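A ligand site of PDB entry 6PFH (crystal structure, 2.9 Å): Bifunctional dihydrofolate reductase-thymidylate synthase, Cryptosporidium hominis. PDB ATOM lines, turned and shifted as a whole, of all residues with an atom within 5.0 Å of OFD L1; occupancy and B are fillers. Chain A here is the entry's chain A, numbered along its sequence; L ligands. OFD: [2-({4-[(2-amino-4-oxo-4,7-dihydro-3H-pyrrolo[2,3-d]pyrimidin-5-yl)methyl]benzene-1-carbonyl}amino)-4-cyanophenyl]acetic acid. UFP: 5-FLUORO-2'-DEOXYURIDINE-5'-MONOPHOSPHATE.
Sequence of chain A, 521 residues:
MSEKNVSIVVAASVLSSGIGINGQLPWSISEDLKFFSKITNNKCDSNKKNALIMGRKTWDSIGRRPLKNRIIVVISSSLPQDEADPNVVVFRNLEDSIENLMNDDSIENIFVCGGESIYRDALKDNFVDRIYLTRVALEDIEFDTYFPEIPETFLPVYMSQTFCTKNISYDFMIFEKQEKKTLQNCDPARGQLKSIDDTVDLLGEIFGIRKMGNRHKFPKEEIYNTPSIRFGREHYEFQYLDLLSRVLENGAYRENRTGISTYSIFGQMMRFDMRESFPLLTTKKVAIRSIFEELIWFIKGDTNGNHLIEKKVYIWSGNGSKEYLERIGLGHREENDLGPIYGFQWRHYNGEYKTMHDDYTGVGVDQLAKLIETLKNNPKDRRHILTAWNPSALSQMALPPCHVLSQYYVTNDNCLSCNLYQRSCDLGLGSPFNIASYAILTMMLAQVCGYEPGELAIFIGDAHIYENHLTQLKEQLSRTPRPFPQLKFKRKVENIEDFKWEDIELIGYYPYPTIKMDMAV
A nitrogen (N3) of OFD L1 is in hydrogen-bond range of the side-chain amide oxygen (OD1) of Asn 319, 2.9 Å away.
O of Ala 520 sits at hydrogen-bond distance from N4 of OFD L1 (3.2 Å).
The side-chain carboxylate (OD2) of Asp 426 lies within hydrogen-bond range of a nitrogen (N1) of OFD L1, 3.4 Å away.
N of Gly 430 sits at hydrogen-bond distance from O1 of OFD L1 (3.4 Å).
N2 of OFD L1 sits close to SD of Met 519, 3.7 Å away.
An oxygen (O2) of UFP L2 lies within hydrogen-bond range of the backbone NH of Asp 426 (2.8 Å).
An oxygen (O3') of UFP L2 lies within hydrogen-bond range of the side-chain hydroxyl (OH) of Tyr 466, 2.5 Å away.
An oxygen (O1P) of UFP L2 is in salt-bridge range of the guanidinium group (NE) of Arg 257 (3.1 Å).
N1 of OFD L1 sits close to O4' of UFP L2 (3.3 Å).
The side-chain amide oxygen (OD1) of Asn 319 sits close to the side-chain sulfur (SD) of Met 519 (3.8 Å).
The indole nitrogen (NE1) of Trp 316 lies within hydrogen-bond range of the side-chain carboxylate (OE2) of Glu 294.
The backbone carbonyl oxygen (O) of Ile 515 lies close to a nitrogen (N6) of OFD L1 (2.9 Å).
Merely in contact with OFD L1: Ala 287 (3.2 Å), Lys 284 (3.2 Å), Ile 315 (3.4 Å), Phe 433 (3.5 Å), Tyr 466 (3.5 Å), Ser 290 (3.5 Å), Leu 399 (3.5 Å), Leu 429 (3.6 Å), Met 517 (3.9 Å) and Trp 316 (3.98 Å).
Hydrophobic or aromatic side chains within 4 Å of OFD L1: Ala 287, Ile 315, Trp 316, Leu 399, Leu 429, Phe 433, Met 517 and Met 519.
Within 4 Å of OFD L1: Lys 284, Ala 287, Ser 290, Ile 315, Trp 316, Asn 319, Leu 399, Asp 426, Leu 429, Gly 430, Phe 433, Tyr 466, Ile 515, Met 517, Met 519 and Ala 520.
Along chain A the residues within 4 Å of OFD L1 span positions 284 to 520.
The nearest printed residue that does not touch OFD L1 is Tyr 314 (4.2 Å).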
ATOM      1  N   ARG A 257     -24.473  -6.437  13.062  1.00  0.00           N
ATOM      2  CA  ARG A 257     -25.735  -6.589  12.342  1.00  0.00           C
ATOM      3  C   ARG A 257     -25.529  -7.101  10.920  1.00  0.00           C
ATOM      4  O   ARG A 257     -26.434  -7.718  10.350  1.00  0.00           O
ATOM      5  CB  ARG A 257     -26.484  -5.253  12.314  1.00  0.00           C
ATOM      6  CG  ARG A 257     -25.670  -4.118  11.718  1.00  0.00           C
ATOM      7  CD  ARG A 257     -26.507  -2.873  11.485  1.00  0.00           C
ATOM      8  NE  ARG A 257     -25.723  -1.882  10.753  1.00  0.00           N
ATOM      9  CZ  ARG A 257     -25.625  -1.843   9.436  1.00  0.00           C
ATOM     10  NH1 ARG A 257     -26.272  -2.737   8.700  1.00  0.00           N
ATOM     11  NH2 ARG A 257     -24.899  -0.906   8.840  1.00  0.00           N
ATOM     12  N   LYS A 284      -3.827   6.762   0.237  1.00  0.00           N
ATOM     13  CA  LYS A 284      -4.891   6.181  -0.564  1.00  0.00           C
ATOM     14  C   LYS A 284      -5.658   7.295  -1.262  1.00  0.00           C
ATOM     15  O   LYS A 284      -5.980   8.317  -0.651  1.00  0.00           O
ATOM     16  CB  LYS A 284      -5.838   5.363   0.330  1.00  0.00           C
ATOM     17  CG  LYS A 284      -7.084   4.873  -0.381  1.00  0.00           C
ATOM     18  CD  LYS A 284      -8.002   4.151   0.592  1.00  0.00           C
ATOM     19  CE  LYS A 284      -8.699   5.134   1.528  1.00  0.00           C
ATOM     20  NZ  LYS A 284      -9.722   4.455   2.380  1.00  0.00           N
ATOM     21  N   LYS A 285      -5.938   7.123  -2.555  1.00  0.00           N
ATOM     22  CA  LYS A 285      -6.712   8.117  -3.280  1.00  0.00           C
ATOM     23  C   LYS A 285      -8.146   8.104  -2.763  1.00  0.00           C
ATOM     24  O   LYS A 285      -8.829   7.075  -2.848  1.00  0.00           O
ATOM     25  CB  LYS A 285      -6.666   7.848  -4.784  1.00  0.00           C
ATOM     26  CG  LYS A 285      -7.265   8.948  -5.640  1.00  0.00           C
ATOM     27  CD  LYS A 285      -7.100   8.652  -7.130  1.00  0.00           C
ATOM     28  CE  LYS A 285      -7.686   9.757  -7.987  1.00  0.00           C
ATOM     29  NZ  LYS A 285      -7.453   9.531  -9.442  1.00  0.00           N
ATOM     30  N   ALA A 287     -12.030   9.627  -2.788  1.00  0.00           N
ATOM     31  CA  ALA A 287     -12.999  10.278  -3.657  1.00  0.00           C
ATOM     32  C   ALA A 287     -13.494  11.577  -3.023  1.00  0.00           C
ATOM     33  O   ALA A 287     -14.522  11.586  -2.339  1.00  0.00           O
ATOM     34  CB  ALA A 287     -14.170   9.344  -3.951  1.00  0.00           C
ATOM     35  N   SER A 290     -17.172  12.776  -4.143  1.00  0.00           N
ATOM     36  CA  SER A 290     -18.285  12.104  -3.492  1.00  0.00           C
ATOM     37  C   SER A 290     -18.474  12.592  -2.067  1.00  0.00           C
ATOM     38  O   SER A 290     -19.599  12.699  -1.583  1.00  0.00           O
ATOM     39  CB  SER A 290     -18.074  10.588  -3.525  1.00  0.00           C
ATOM     40  OG  SER A 290     -17.861  10.138  -4.846  1.00  0.00           O
ATOM     41  N   GLU A 294     -21.992  14.435  -0.880  1.00  0.00           N
ATOM     42  CA  GLU A 294     -22.738  13.976   0.281  1.00  0.00           C
ATOM     43  C   GLU A 294     -22.925  15.095   1.297  1.00  0.00           C
ATOM     44  O   GLU A 294     -23.981  15.214   1.914  1.00  0.00           O
ATOM     45  CB  GLU A 294     -22.030  12.789   0.939  1.00  0.00           C
ATOM     46  CG  GLU A 294     -22.752  12.226   2.160  1.00  0.00           C
ATOM     47  CD  GLU A 294     -21.835  11.429   3.064  1.00  0.00           C
ATOM     48  OE1 GLU A 294     -20.658  11.808   3.200  1.00  0.00           O
ATOM     49  OE2 GLU A 294     -22.295  10.419   3.640  1.00  0.00           O
ATOM     50  N   VAL A 313     -22.780   9.265  -7.396  1.00  0.00           N
ATOM     51  CA  VAL A 313     -22.346   9.022  -6.020  1.00  0.00           C
ATOM     52  C   VAL A 313     -23.170   7.860  -5.488  1.00  0.00           C
ATOM     53  O   VAL A 313     -24.396   7.987  -5.331  1.00  0.00           O
ATOM     54  CB  VAL A 313     -22.484  10.259  -5.132  1.00  0.00           C
ATOM     55  CG1 VAL A 313     -22.117   9.932  -3.700  1.00  0.00           C
ATOM     56  CG2 VAL A 313     -21.600  11.370  -5.657  1.00  0.00           C
ATOM     57  N   TYR A 314     -22.513   6.733  -5.198  1.00  0.00           N
ATOM     58  CA  TYR A 314     -23.211   5.498  -4.862  1.00  0.00           C
ATOM     59  C   TYR A 314     -22.900   5.023  -3.445  1.00  0.00           C
ATOM     60  O   TYR A 314     -22.984   3.833  -3.153  1.00  0.00           O
ATOM     61  CB  TYR A 314     -22.847   4.400  -5.854  1.00  0.00           C
ATOM     62  CG  TYR A 314     -22.891   4.810  -7.311  1.00  0.00           C
ATOM     63  CD1 TYR A 314     -24.098   4.884  -8.000  1.00  0.00           C
ATOM     64  CD2 TYR A 314     -21.731   5.135  -7.997  1.00  0.00           C
ATOM     65  CE1 TYR A 314     -24.140   5.247  -9.326  1.00  0.00           C
ATOM     66  CE2 TYR A 314     -21.763   5.508  -9.332  1.00  0.00           C
ATOM     67  CZ  TYR A 314     -22.969   5.569  -9.993  1.00  0.00           C
ATOM     68  OH  TYR A 314     -23.015   5.942 -11.310  1.00  0.00           O
ATOM     69  N   ILE A 315     -22.561   5.942  -2.530  1.00  0.00           N
ATOM     70  CA  ILE A 315     -22.206   5.512  -1.187  1.00  0.00           C
ATOM     71  C   ILE A 315     -23.426   5.164  -0.343  1.00  0.00           C
ATOM     72  O   ILE A 315     -23.311   4.370   0.605  1.00  0.00           O
ATOM     73  CB  ILE A 315     -21.358   6.569  -0.466  1.00  0.00           C
ATOM     74  CG1 ILE A 315     -22.159   7.850  -0.222  1.00  0.00           C
ATOM     75  CG2 ILE A 315     -20.090   6.866  -1.260  1.00  0.00           C
ATOM     76  CD1 ILE A 315     -21.394   8.883   0.576  1.00  0.00           C
ATOM     77  N   TRP A 316     -24.598   5.708  -0.657  1.00  0.00           N
ATOM     78  CA  TRP A 316     -25.829   5.397   0.064  1.00  0.00           C
ATOM     79  C   TRP A 316     -26.749   4.469  -0.708  1.00  0.00           C
ATOM     80  O   TRP A 316     -27.949   4.428  -0.433  1.00  0.00           O
ATOM     81  CB  TRP A 316     -26.578   6.677   0.439  1.00  0.00           C
ATOM     82  CG  TRP A 316     -25.959   7.446   1.567  1.00  0.00           C
ATOM     83  CD1 TRP A 316     -25.156   8.536   1.472  1.00  0.00           C
ATOM     84  CD2 TRP A 316     -26.107   7.173   2.972  1.00  0.00           C
ATOM     85  NE1 TRP A 316     -24.791   8.961   2.728  1.00  0.00           N
ATOM     86  CE2 TRP A 316     -25.354   8.135   3.665  1.00  0.00           C
ATOM     87  CE3 TRP A 316     -26.790   6.198   3.703  1.00  0.00           C
ATOM     88  CZ2 TRP A 316     -25.277   8.171   5.055  1.00  0.00           C
ATOM     89  CZ3 TRP A 316     -26.709   6.224   5.085  1.00  0.00           C
ATOM     90  CH2 TRP A 316     -25.957   7.199   5.750  1.00  0.00           C
ATOM     91  N   ASN A 319     -27.450   0.988   1.739  1.00  0.00           N
ATOM     92  CA  ASN A 319     -28.406   1.189   2.813  1.00  0.00           C
ATOM     93  C   ASN A 319     -29.733   1.770   2.317  1.00  0.00           C
ATOM     94  O   ASN A 319     -30.582   2.121   3.140  1.00  0.00           O
ATOM     95  CB  ASN A 319     -27.809   2.094   3.890  1.00  0.00           C
ATOM     96  CG  ASN A 319     -26.461   1.604   4.351  1.00  0.00           C
ATOM     97  OD1 ASN A 319     -25.425   1.986   3.811  1.00  0.00           O
ATOM     98  ND2 ASN A 319     -26.454   0.732   5.363  1.00  0.00           N
ATOM     99  N   LEU A 399     -30.506   4.147   8.535  1.00  0.00           N
ATOM    100  CA  LEU A 399     -29.312   3.864   9.316  1.00  0.00           C
ATOM    101  C   LEU A 399     -29.161   4.938  10.380  1.00  0.00           C
ATOM    102  O   LEU A 399     -29.224   6.126  10.064  1.00  0.00           O
ATOM    103  CB  LEU A 399     -28.078   3.808   8.412  1.00  0.00           C
ATOM    104  CG  LEU A 399     -26.807   3.225   9.040  1.00  0.00           C
ATOM    105  CD1 LEU A 399     -27.019   1.752   9.354  1.00  0.00           C
ATOM    106  CD2 LEU A 399     -25.607   3.418   8.126  1.00  0.00           C
ATOM    107  N   ASP A 426     -16.229   2.878  10.675  1.00  0.00           N
ATOM    108  CA  ASP A 426     -15.612   1.988   9.692  1.00  0.00           C
ATOM    109  C   ASP A 426     -14.298   2.611   9.249  1.00  0.00           C
ATOM    110  O   ASP A 426     -14.289   3.551   8.452  1.00  0.00           O
ATOM    111  CB  ASP A 426     -16.562   1.772   8.513  1.00  0.00           C
ATOM    112  CG  ASP A 426     -16.001   0.818   7.470  1.00  0.00           C
ATOM    113  OD1 ASP A 426     -14.882   0.300   7.657  1.00  0.00           O
ATOM    114  OD2 ASP A 426     -16.703   0.578   6.462  1.00  0.00           O
ATOM    115  N   LEU A 429     -13.618   2.621   5.173  1.00  0.00           N
ATOM    116  CA  LEU A 429     -14.373   3.448   4.242  1.00  0.00           C
ATOM    117  C   LEU A 429     -14.925   4.718   4.877  1.00  0.00           C
ATOM    118  O   LEU A 429     -14.678   5.814   4.361  1.00  0.00           O
ATOM    119  CB  LEU A 429     -15.537   2.633   3.647  1.00  0.00           C
ATOM    120  CG  LEU A 429     -15.171   1.386   2.845  1.00  0.00           C
ATOM    121  CD1 LEU A 429     -16.418   0.697   2.327  1.00  0.00           C
ATOM    122  CD2 LEU A 429     -14.241   1.738   1.708  1.00  0.00           C
ATOM    123  N   GLY A 430     -15.647   4.601   5.993  1.00  0.00           N
ATOM    124  CA  GLY A 430     -16.318   5.769   6.541  1.00  0.00           C
ATOM    125  C   GLY A 430     -15.378   6.779   7.159  1.00  0.00           C
ATOM    126  O   GLY A 430     -15.590   7.986   7.050  1.00  0.00           O
ATOM    127  N   PHE A 433     -13.743   9.394   4.836  1.00  0.00           N
ATOM    128  CA  PHE A 433     -14.830  10.269   4.423  1.00  0.00           C
ATOM    129  C   PHE A 433     -15.231  11.224   5.534  1.00  0.00           C
ATOM    130  O   PHE A 433     -15.411  12.417   5.303  1.00  0.00           O
ATOM    131  CB  PHE A 433     -16.019   9.434   3.962  1.00  0.00           C
ATOM    132  CG  PHE A 433     -15.968   9.034   2.521  1.00  0.00           C
ATOM    133  CD1 PHE A 433     -14.854   8.387   2.008  1.00  0.00           C
ATOM    134  CD2 PHE A 433     -17.032   9.284   1.670  1.00  0.00           C
ATOM    135  CE1 PHE A 433     -14.804   8.014   0.672  1.00  0.00           C
ATOM    136  CE2 PHE A 433     -16.990   8.914   0.340  1.00  0.00           C
ATOM    137  CZ  PHE A 433     -15.868   8.270  -0.162  1.00  0.00           C
ATOM    138  N   TYR A 466     -13.404  -4.017   9.338  1.00  0.00           N
ATOM    139  CA  TYR A 466     -14.113  -5.179   8.810  1.00  0.00           C
ATOM    140  C   TYR A 466     -13.117  -6.211   8.309  1.00  0.00           C
ATOM    141  O   TYR A 466     -12.083  -5.872   7.729  1.00  0.00           O
ATOM    142  CB  TYR A 466     -15.072  -4.759   7.695  1.00  0.00           C
ATOM    143  CG  TYR A 466     -16.340  -4.125   8.218  1.00  0.00           C
ATOM    144  CD1 TYR A 466     -16.410  -2.758   8.451  1.00  0.00           C
ATOM    145  CD2 TYR A 466     -17.467  -4.891   8.485  1.00  0.00           C
ATOM    146  CE1 TYR A 466     -17.569  -2.173   8.940  1.00  0.00           C
ATOM    147  CE2 TYR A 466     -18.628  -4.318   8.978  1.00  0.00           C
ATOM    148  CZ  TYR A 466     -18.673  -2.960   9.197  1.00  0.00           C
ATOM    149  OH  TYR A 466     -19.831  -2.398   9.682  1.00  0.00           O
ATOM    150  N   THR A 514      -5.643   4.038  -5.589  1.00  0.00           N
ATOM    151  CA  THR A 514      -6.872   3.697  -4.889  1.00  0.00           C
ATOM    152  C   THR A 514      -6.819   2.256  -4.386  1.00  0.00           C
ATOM    153  O   THR A 514      -6.134   1.406  -4.966  1.00  0.00           O
ATOM    154  CB  THR A 514      -8.091   3.880  -5.803  1.00  0.00           C
ATOM    155  OG1 THR A 514      -7.994   5.138  -6.482  1.00  0.00           O
ATOM    156  CG2 THR A 514      -9.392   3.850  -5.007  1.00  0.00           C
ATOM    157  N   ILE A 515      -7.509   2.002  -3.285  1.00  0.00           N
ATOM    158  CA  ILE A 515      -7.591   0.672  -2.685  1.00  0.00           C
ATOM    159  C   ILE A 515      -9.071   0.317  -2.592  1.00  0.00           C
ATOM    160  O   ILE A 515      -9.806   0.928  -1.802  1.00  0.00           O
ATOM    161  CB  ILE A 515      -6.917   0.614  -1.311  1.00  0.00           C
ATOM    162  CG1 ILE A 515      -5.437   0.963  -1.420  1.00  0.00           C
ATOM    163  CG2 ILE A 515      -7.082  -0.757  -0.707  1.00  0.00           C
ATOM    164  CD1 ILE A 515      -4.717   0.988  -0.096  1.00  0.00           C
ATOM    165  N   MET A 517     -12.394  -1.403  -1.541  1.00  0.00           N
ATOM    166  CA  MET A 517     -12.915  -2.070  -0.351  1.00  0.00           C
ATOM    167  C   MET A 517     -14.435  -2.080  -0.416  1.00  0.00           C
ATOM    168  O   MET A 517     -15.045  -1.042  -0.681  1.00  0.00           O
ATOM    169  CB  MET A 517     -12.446  -1.367   0.927  1.00  0.00           C
ATOM    170  CG  MET A 517     -11.003  -1.673   1.325  1.00  0.00           C
ATOM    171  SD  MET A 517     -10.399  -0.630   2.667  1.00  0.00           S
ATOM    172  CE  MET A 517     -10.185   0.938   1.812  1.00  0.00           C
ATOM    173  N   MET A 519     -18.301  -2.353   0.920  1.00  0.00           N
ATOM    174  CA  MET A 519     -19.075  -1.938   2.083  1.00  0.00           C
ATOM    175  C   MET A 519     -19.929  -3.087   2.598  1.00  0.00           C
ATOM    176  O   MET A 519     -20.509  -3.852   1.822  1.00  0.00           O
ATOM    177  CB  MET A 519     -19.968  -0.750   1.745  1.00  0.00           C
ATOM    178  CG  MET A 519     -20.873  -0.338   2.892  1.00  0.00           C
ATOM    179  SD  MET A 519     -22.027   0.965   2.475  1.00  0.00           S
ATOM    180  CE  MET A 519     -23.068   0.107   1.292  1.00  0.00           C
ATOM    181  N   ALA A 520     -20.023  -3.193   3.919  1.00  0.00           N
ATOM    182  CA  ALA A 520     -20.874  -4.189   4.559  1.00  0.00           C
ATOM    183  C   ALA A 520     -22.288  -3.632   4.670  1.00  0.00           C
ATOM    184  O   ALA A 520     -22.524  -2.634   5.359  1.00  0.00           O
ATOM    185  CB  ALA A 520     -20.339  -4.565   5.934  1.00  0.00           C
HETATM  186  O1  OFD L   1     -18.827   3.491   5.589  1.00  0.00           O
HETATM  187  C1  OFD L   1     -21.088   0.901   6.411  1.00  0.00           C
HETATM  188  O2  OFD L   1     -17.865   3.054  -0.622  1.00  0.00           O
HETATM  189  C2  OFD L   1     -22.307   2.662   5.670  1.00  0.00           C
HETATM  190  C3  OFD L   1     -21.209   3.451   5.443  1.00  0.00           C
HETATM  191  C4  OFD L   1     -19.884   2.869   5.750  1.00  0.00           C
HETATM  192  C5  OFD L   1     -21.684   4.702   4.943  1.00  0.00           C
HETATM  193  C6  OFD L   1     -23.059   4.620   4.877  1.00  0.00           C
HETATM  194  C7  OFD L   1     -20.866   5.889   4.531  1.00  0.00           C
HETATM  195  C8  OFD L   1     -20.017   5.442   3.368  1.00  0.00           C
HETATM  196  C9  OFD L   1     -20.519   4.476   2.468  1.00  0.00           C
HETATM  197  C10 OFD L   1     -19.729   4.040   1.385  1.00  0.00           C
HETATM  198  C11 OFD L   1     -18.434   4.560   1.194  1.00  0.00           C
HETATM  199  C12 OFD L   1     -17.925   5.510   2.094  1.00  0.00           C
HETATM  200  O3  OFD L   1     -18.346   6.655  -4.441  1.00  0.00           O
HETATM  201  C13 OFD L   1     -18.710   5.954   3.181  1.00  0.00           C
HETATM  202  C14 OFD L   1     -17.609   4.060   0.042  1.00  0.00           C
HETATM  203  C15 OFD L   1     -15.558   4.598  -1.255  1.00  0.00           C
HETATM  204  C16 OFD L   1     -15.864   4.618  -2.637  1.00  0.00           C
HETATM  205  C17 OFD L   1     -14.854   4.367  -3.590  1.00  0.00           C
HETATM  206  C18 OFD L   1     -13.532   4.098  -3.173  1.00  0.00           C
HETATM  207  C19 OFD L   1     -13.225   4.078  -1.790  1.00  0.00           C
HETATM  208  C20 OFD L   1     -14.240   4.321  -0.842  1.00  0.00           C
HETATM  209  C21 OFD L   1     -11.825   3.796  -1.335  1.00  0.00           C
HETATM  210  C22 OFD L   1     -17.266   4.900  -3.117  1.00  0.00           C
HETATM  211  C23 OFD L   1     -17.353   6.192  -3.882  1.00  0.00           C
HETATM  212  N1  OFD L   1     -19.898   1.621   6.217  1.00  0.00           N
HETATM  213  N2  OFD L   1     -22.287   1.357   6.163  1.00  0.00           N
HETATM  214  N3  OFD L   1     -23.431   3.363   5.331  1.00  0.00           N
HETATM  215  N4  OFD L   1     -20.881  -0.441   6.936  1.00  0.00           N
HETATM  216  N5  OFD L   1     -16.555   4.838  -0.214  1.00  0.00           N
HETATM  217  N6  OFD L   1     -10.749   3.573  -0.974  1.00  0.00           N
HETATM  218  O4  OFD L   1     -16.139   6.804  -3.893  1.00  0.00           O
HETATM  219  N1  UFP L   2     -20.061   4.344   8.998  1.00  0.00           N
HETATM  220  C2  UFP L   2     -19.056   5.209   9.333  1.00  0.00           C
HETATM  221  N3  UFP L   2     -19.166   6.520   9.053  1.00  0.00           N
HETATM  222  C4  UFP L   2     -20.254   7.014   8.438  1.00  0.00           C
HETATM  223  C5  UFP L   2     -21.300   6.134   8.083  1.00  0.00           C
HETATM  224  C6  UFP L   2     -21.166   4.820   8.364  1.00  0.00           C
HETATM  225  O2  UFP L   2     -18.031   4.858   9.904  1.00  0.00           O
HETATM  226  O4  UFP L   2     -20.338   8.211   8.185  1.00  0.00           O
HETATM  227  F5  UFP L   2     -22.409   6.583   7.457  1.00  0.00           F
HETATM  228  C1' UFP L   2     -20.063   2.889   9.247  1.00  0.00           C
HETATM  229  C2' UFP L   2     -19.721   2.458  10.694  1.00  0.00           C
HETATM  230  C3' UFP L   2     -20.348   1.055  10.729  1.00  0.00           C
HETATM  231  C4' UFP L   2     -21.653   1.255   9.946  1.00  0.00           C
HETATM  232  O3' UFP L   2     -19.523   0.102  10.056  1.00  0.00           O
HETATM  233  O4' UFP L   2     -21.427   2.397   9.080  1.00  0.00           O
HETATM  234  C5' UFP L   2     -22.821   1.498  10.901  1.00  0.00           C
HETATM  235  O5' UFP L   2     -23.391   0.238  11.263  1.00  0.00           O
HETATM  236  P   UFP L   2     -23.898   0.345  12.788  1.00  0.00           P
HETATM  237  O1P UFP L   2     -24.170  -1.130  13.349  1.00  0.00           O
HETATM  238  O2P UFP L   2     -22.849   0.987  13.612  1.00  0.00           O
HETATM  239  O3P UFP L   2     -25.245   1.217  12.859  1.00  0.00           O
